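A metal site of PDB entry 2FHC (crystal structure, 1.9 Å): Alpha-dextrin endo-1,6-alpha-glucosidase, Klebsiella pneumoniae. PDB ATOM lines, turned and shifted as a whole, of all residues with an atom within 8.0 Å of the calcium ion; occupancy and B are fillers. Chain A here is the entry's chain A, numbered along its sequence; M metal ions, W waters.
Within 4 Å of the calcium ion: Ala 550, Asp 553, Tyr 555 and Asp 893.
Along chain A the residues within 4 Å of the calcium ion span positions 550 to 893.
O of Tyr 555 is bound to the calcium ion.
The side-chain carboxylate (OD2) of Asp 893 is bound to the calcium ion (2.4 Å).
O of Ala 550 is bound to the calcium ion, 2.4 Å away.
OD1 of Asp 553 binds the calcium ion (2.4 Å).
The calcium ion is bound by water W1 (2.4 Å).
The calcium ion is bound by water W2 (2.6 Å).
The calcium ion is bound by water W3 (2.6 Å).
The calcium ion has seven donor atoms within binding distance.
Water W2 lies within hydrogen-bond range of the backbone carbonyl oxygen (O) of Thr 484 and the side-chain amide nitrogen (ND2) of Asn 556.
Water W1 bridges the backbone carbonyl oxygen (O) of Asp 553 and the backbone carbonyl oxygen (O) of Thr 484.
Water W3 lies within hydrogen-bond range of the side-chain carboxylate (OD2) of Asp 553 (2.7 Å), the backbone carbonyl oxygen (O) of Asp 893 (3.0 Å) and the backbone NH (N) of Gly 895 (3.2 Å).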
ATOM      1  N   THR A 484      20.240  21.681 -27.545  1.00  0.00           N
ATOM      2  CA  THR A 484      20.063  20.875 -26.346  1.00  0.00           C
ATOM      3  C   THR A 484      19.346  19.517 -26.379  1.00  0.00           C
ATOM      4  O   THR A 484      18.937  19.001 -25.331  1.00  0.00           O
ATOM      5  CB  THR A 484      19.467  21.758 -25.247  1.00  0.00           C
ATOM      6  OG1 THR A 484      18.395  22.538 -25.774  1.00  0.00           O
ATOM      7  CG2 THR A 484      20.545  22.713 -24.718  1.00  0.00           C
ATOM      8  N   VAL A 485      19.215  18.945 -27.575  1.00  0.00           N
ATOM      9  CA  VAL A 485      18.631  17.614 -27.755  1.00  0.00           C
ATOM     10  C   VAL A 485      19.529  16.879 -28.763  1.00  0.00           C
ATOM     11  O   VAL A 485      19.765  17.378 -29.859  1.00  0.00           O
ATOM     12  CB  VAL A 485      17.195  17.656 -28.323  1.00  0.00           C
ATOM     13  CG1 VAL A 485      16.763  16.248 -28.776  1.00  0.00           C
ATOM     14  CG2 VAL A 485      16.218  18.168 -27.260  1.00  0.00           C
ATOM     15  N   ASN A 486      20.045  15.711 -28.384  1.00  0.00           N
ATOM     16  CA  ASN A 486      20.920  14.968 -29.294  1.00  0.00           C
ATOM     17  C   ASN A 486      20.065  14.344 -30.398  1.00  0.00           C
ATOM     18  O   ASN A 486      19.100  13.629 -30.121  1.00  0.00           O
ATOM     19  CB  ASN A 486      21.672  13.871 -28.528  1.00  0.00           C
ATOM     20  CG  ASN A 486      22.881  13.348 -29.304  1.00  0.00           C
ATOM     21  OD1 ASN A 486      22.773  12.999 -30.479  1.00  0.00           O
ATOM     22  ND2 ASN A 486      24.025  13.294 -28.643  1.00  0.00           N
ATOM     23  N   ASP A 494      14.042   7.938 -23.753  1.00  0.00           N
ATOM     24  CA  ASP A 494      12.849   8.639 -23.280  1.00  0.00           C
ATOM     25  C   ASP A 494      12.092   7.792 -22.249  1.00  0.00           C
ATOM     26  O   ASP A 494      12.306   6.577 -22.154  1.00  0.00           O
ATOM     27  CB  ASP A 494      11.974   9.016 -24.475  1.00  0.00           C
ATOM     28  CG  ASP A 494      12.548  10.209 -25.238  1.00  0.00           C
ATOM     29  OD1 ASP A 494      12.631  11.305 -24.637  1.00  0.00           O
ATOM     30  OD2 ASP A 494      12.921  10.067 -26.427  1.00  0.00           O
ATOM     31  N   ASN A 546      13.920  12.259 -12.364  1.00  0.00           N
ATOM     32  CA  ASN A 546      13.652  13.007 -13.586  1.00  0.00           C
ATOM     33  C   ASN A 546      14.792  13.962 -13.952  1.00  0.00           C
ATOM     34  O   ASN A 546      15.067  14.185 -15.130  1.00  0.00           O
ATOM     35  CB  ASN A 546      12.340  13.783 -13.471  1.00  0.00           C
ATOM     36  CG  ASN A 546      11.770  14.162 -14.832  1.00  0.00           C
ATOM     37  OD1 ASN A 546      11.577  13.292 -15.686  1.00  0.00           O
ATOM     38  ND2 ASN A 546      11.485  15.439 -15.031  1.00  0.00           N
ATOM     39  N   THR A 547      15.450  14.525 -12.937  1.00  0.00           N
ATOM     40  CA  THR A 547      16.551  15.440 -13.182  1.00  0.00           C
ATOM     41  C   THR A 547      17.664  14.744 -13.970  1.00  0.00           C
ATOM     42  O   THR A 547      18.362  15.370 -14.769  1.00  0.00           O
ATOM     43  CB  THR A 547      17.112  15.999 -11.861  1.00  0.00           C
ATOM     44  OG1 THR A 547      16.127  16.862 -11.270  1.00  0.00           O
ATOM     45  CG2 THR A 547      18.399  16.802 -12.104  1.00  0.00           C
ATOM     46  N   LEU A 548      17.831  13.445 -13.728  1.00  0.00           N
ATOM     47  CA  LEU A 548      18.839  12.680 -14.434  1.00  0.00           C
ATOM     48  C   LEU A 548      18.339  12.344 -15.841  1.00  0.00           C
ATOM     49  O   LEU A 548      19.081  12.462 -16.814  1.00  0.00           O
ATOM     50  CB  LEU A 548      19.154  11.383 -13.673  1.00  0.00           C
ATOM     51  CG  LEU A 548      19.682  11.614 -12.250  1.00  0.00           C
ATOM     52  CD1 LEU A 548      19.939  10.283 -11.550  1.00  0.00           C
ATOM     53  CD2 LEU A 548      20.975  12.433 -12.314  1.00  0.00           C
ATOM     54  N   VAL A 549      17.075  11.951 -15.933  1.00  0.00           N
ATOM     55  CA  VAL A 549      16.458  11.627 -17.224  1.00  0.00           C
ATOM     56  C   VAL A 549      16.533  12.812 -18.204  1.00  0.00           C
ATOM     57  O   VAL A 549      16.766  12.628 -19.408  1.00  0.00           O
ATOM     58  CB  VAL A 549      14.957  11.245 -17.035  1.00  0.00           C
ATOM     59  CG1 VAL A 549      14.266  11.123 -18.399  1.00  0.00           C
ATOM     60  CG2 VAL A 549      14.854   9.916 -16.279  1.00  0.00           C
ATOM     61  N   ALA A 550      16.365  14.016 -17.678  1.00  0.00           N
ATOM     62  CA  ALA A 550      16.382  15.238 -18.492  1.00  0.00           C
ATOM     63  C   ALA A 550      17.669  15.451 -19.297  1.00  0.00           C
ATOM     64  O   ALA A 550      17.656  16.115 -20.334  1.00  0.00           O
ATOM     65  CB  ALA A 550      16.119  16.440 -17.597  1.00  0.00           C
ATOM     66  N   GLN A 551      18.764  14.876 -18.818  1.00  0.00           N
ATOM     67  CA  GLN A 551      20.068  15.025 -19.477  1.00  0.00           C
ATOM     68  C   GLN A 551      20.191  14.322 -20.816  1.00  0.00           C
ATOM     69  O   GLN A 551      20.921  14.775 -21.698  1.00  0.00           O
ATOM     70  CB  GLN A 551      21.174  14.496 -18.547  1.00  0.00           C
ATOM     71  CG  GLN A 551      21.241  15.172 -17.196  1.00  0.00           C
ATOM     72  CD  GLN A 551      22.133  14.432 -16.223  1.00  0.00           C
ATOM     73  OE1 GLN A 551      22.461  14.954 -15.152  1.00  0.00           O
ATOM     74  NE2 GLN A 551      22.535  13.221 -16.583  1.00  0.00           N
ATOM     75  N   THR A 552      19.469  13.216 -20.984  1.00  0.00           N
ATOM     76  CA  THR A 552      19.555  12.439 -22.210  1.00  0.00           C
ATOM     77  C   THR A 552      18.235  12.105 -22.898  1.00  0.00           C
ATOM     78  O   THR A 552      18.179  11.151 -23.670  1.00  0.00           O
ATOM     79  CB  THR A 552      20.318  11.104 -21.954  1.00  0.00           C
ATOM     80  OG1 THR A 552      19.788  10.457 -20.791  1.00  0.00           O
ATOM     81  CG2 THR A 552      21.793  11.365 -21.724  1.00  0.00           C
ATOM     82  N   ASP A 553      17.187  12.874 -22.632  1.00  0.00           N
ATOM     83  CA  ASP A 553      15.897  12.620 -23.282  1.00  0.00           C
ATOM     84  C   ASP A 553      15.729  13.498 -24.528  1.00  0.00           C
ATOM     85  O   ASP A 553      16.661  14.196 -24.923  1.00  0.00           O
ATOM     86  CB  ASP A 553      14.724  12.843 -22.302  1.00  0.00           C
ATOM     87  CG  ASP A 553      14.645  14.274 -21.762  1.00  0.00           C
ATOM     88  OD1 ASP A 553      15.357  15.167 -22.265  1.00  0.00           O
ATOM     89  OD2 ASP A 553      13.852  14.492 -20.823  1.00  0.00           O
ATOM     90  N   SER A 554      14.555  13.439 -25.154  1.00  0.00           N
ATOM     91  CA  SER A 554      14.300  14.220 -26.366  1.00  0.00           C
ATOM     92  C   SER A 554      13.644  15.565 -26.050  1.00  0.00           C
ATOM     93  O   SER A 554      13.216  16.272 -26.969  1.00  0.00           O
ATOM     94  CB  SER A 554      13.361  13.445 -27.297  1.00  0.00           C
ATOM     95  OG  SER A 554      13.908  12.201 -27.688  1.00  0.00           O
ATOM     96  N   TYR A 555      13.573  15.928 -24.775  1.00  0.00           N
ATOM     97  CA  TYR A 555      12.883  17.140 -24.370  1.00  0.00           C
ATOM     98  C   TYR A 555      13.641  18.411 -23.967  1.00  0.00           C
ATOM     99  O   TYR A 555      14.573  18.367 -23.152  1.00  0.00           O
ATOM    100  CB  TYR A 555      11.910  16.799 -23.227  1.00  0.00           C
ATOM    101  CG  TYR A 555      10.873  17.862 -22.964  1.00  0.00           C
ATOM    102  CD1 TYR A 555      11.209  19.076 -22.360  1.00  0.00           C
ATOM    103  CD2 TYR A 555       9.557  17.701 -23.408  1.00  0.00           C
ATOM    104  CE1 TYR A 555      10.275  20.111 -22.220  1.00  0.00           C
ATOM    105  CE2 TYR A 555       8.616  18.707 -23.272  1.00  0.00           C
ATOM    106  CZ  TYR A 555       8.982  19.912 -22.677  1.00  0.00           C
ATOM    107  OH  TYR A 555       8.053  20.927 -22.593  1.00  0.00           O
ATOM    108  N   ASN A 556      13.205  19.537 -24.534  1.00  0.00           N
ATOM    109  CA  ASN A 556      13.711  20.868 -24.186  1.00  0.00           C
ATOM    110  C   ASN A 556      12.889  21.899 -24.942  1.00  0.00           C
ATOM    111  O   ASN A 556      12.470  21.670 -26.071  1.00  0.00           O
ATOM    112  CB  ASN A 556      15.199  21.035 -24.511  1.00  0.00           C
ATOM    113  CG  ASN A 556      15.829  22.216 -23.770  1.00  0.00           C
ATOM    114  OD1 ASN A 556      15.555  23.371 -24.069  1.00  0.00           O
ATOM    115  ND2 ASN A 556      16.657  21.910 -22.776  1.00  0.00           N
ATOM    116  N   TRP A 557      12.627  23.045 -24.304  1.00  0.00           N
ATOM    117  CA  TRP A 557      11.875  24.104 -24.975  1.00  0.00           C
ATOM    118  C   TRP A 557      12.650  24.514 -26.222  1.00  0.00           C
ATOM    119  O   TRP A 557      12.052  24.868 -27.252  1.00  0.00           O
ATOM    120  CB  TRP A 557      11.710  25.332 -24.073  1.00  0.00           C
ATOM    121  CG  TRP A 557      10.657  25.197 -23.015  1.00  0.00           C
ATOM    122  CD1 TRP A 557       9.675  24.250 -22.927  1.00  0.00           C
ATOM    123  CD2 TRP A 557      10.478  26.071 -21.897  1.00  0.00           C
ATOM    124  NE1 TRP A 557       8.890  24.485 -21.826  1.00  0.00           N
ATOM    125  CE2 TRP A 557       9.358  25.592 -21.169  1.00  0.00           C
ATOM    126  CE3 TRP A 557      11.147  27.215 -21.434  1.00  0.00           C
ATOM    127  CZ2 TRP A 557       8.903  26.218 -20.010  1.00  0.00           C
ATOM    128  CZ3 TRP A 557      10.699  27.829 -20.274  1.00  0.00           C
ATOM    129  CH2 TRP A 557       9.581  27.332 -19.568  1.00  0.00           C
ATOM    130  N   TYR A 892      11.496  24.266 -18.645  1.00  0.00           N
ATOM    131  CA  TYR A 892      12.236  24.094 -19.894  1.00  0.00           C
ATOM    132  C   TYR A 892      12.949  22.760 -20.130  1.00  0.00           C
ATOM    133  O   TYR A 892      13.059  22.313 -21.268  1.00  0.00           O
ATOM    134  CB  TYR A 892      13.258  25.227 -20.068  1.00  0.00           C
ATOM    135  CG  TYR A 892      14.501  25.073 -19.223  1.00  0.00           C
ATOM    136  CD1 TYR A 892      14.465  25.264 -17.840  1.00  0.00           C
ATOM    137  CD2 TYR A 892      15.720  24.728 -19.813  1.00  0.00           C
ATOM    138  CE1 TYR A 892      15.608  25.100 -17.061  1.00  0.00           C
ATOM    139  CE2 TYR A 892      16.870  24.559 -19.040  1.00  0.00           C
ATOM    140  CZ  TYR A 892      16.807  24.758 -17.665  1.00  0.00           C
ATOM    141  OH  TYR A 892      17.944  24.613 -16.911  1.00  0.00           O
ATOM    142  N   ASP A 893      13.427  22.134 -19.062  1.00  0.00           N
ATOM    143  CA  ASP A 893      14.142  20.866 -19.170  1.00  0.00           C
ATOM    144  C   ASP A 893      13.523  19.817 -18.235  1.00  0.00           C
ATOM    145  O   ASP A 893      14.190  18.864 -17.835  1.00  0.00           O
ATOM    146  CB  ASP A 893      15.612  21.076 -18.796  1.00  0.00           C
ATOM    147  CG  ASP A 893      16.523  19.981 -19.312  1.00  0.00           C
ATOM    148  OD1 ASP A 893      17.666  19.891 -18.806  1.00  0.00           O
ATOM    149  OD2 ASP A 893      16.127  19.224 -20.215  1.00  0.00           O
ATOM    150  N   SER A 894      12.243  19.995 -17.899  1.00  0.00           N
ATOM    151  CA  SER A 894      11.554  19.066 -16.996  1.00  0.00           C
ATOM    152  C   SER A 894      10.905  17.872 -17.692  1.00  0.00           C
ATOM    153  O   SER A 894      10.083  17.165 -17.095  1.00  0.00           O
ATOM    154  CB  SER A 894      10.521  19.824 -16.158  1.00  0.00           C
ATOM    155  OG  SER A 894      11.176  20.702 -15.248  1.00  0.00           O
ATOM    156  N   GLY A 895      11.244  17.667 -18.961  1.00  0.00           N
ATOM    157  CA  GLY A 895      10.757  16.535 -19.728  1.00  0.00           C
ATOM    158  C   GLY A 895       9.281  16.299 -19.943  1.00  0.00           C
ATOM    159  O   GLY A 895       8.434  17.142 -19.636  1.00  0.00           O
ATOM    160  N   ASP A 896       8.961  15.127 -20.496  1.00  0.00           N
ATOM    161  CA  ASP A 896       7.591  14.732 -20.771  1.00  0.00           C
ATOM    162  C   ASP A 896       6.739  14.618 -19.500  1.00  0.00           C
ATOM    163  O   ASP A 896       5.539  14.889 -19.536  1.00  0.00           O
ATOM    164  CB  ASP A 896       7.543  13.369 -21.490  1.00  0.00           C
ATOM    165  CG  ASP A 896       8.131  13.402 -22.894  1.00  0.00           C
ATOM    166  OD1 ASP A 896       8.114  14.477 -23.525  1.00  0.00           O
ATOM    167  OD2 ASP A 896       8.583  12.331 -23.364  1.00  0.00           O
HETATM  168 CA    CA M   1      16.198  17.393 -21.750  1.00  0.00          CA
HETATM  169  O   HOH W   1      17.470  16.468 -23.612  1.00  0.00           O
HETATM  170  O   HOH W   2      17.910  19.101 -22.626  1.00  0.00           O
HETATM  171  O   HOH W   3      14.115  17.135 -20.249  1.00  0.00           O
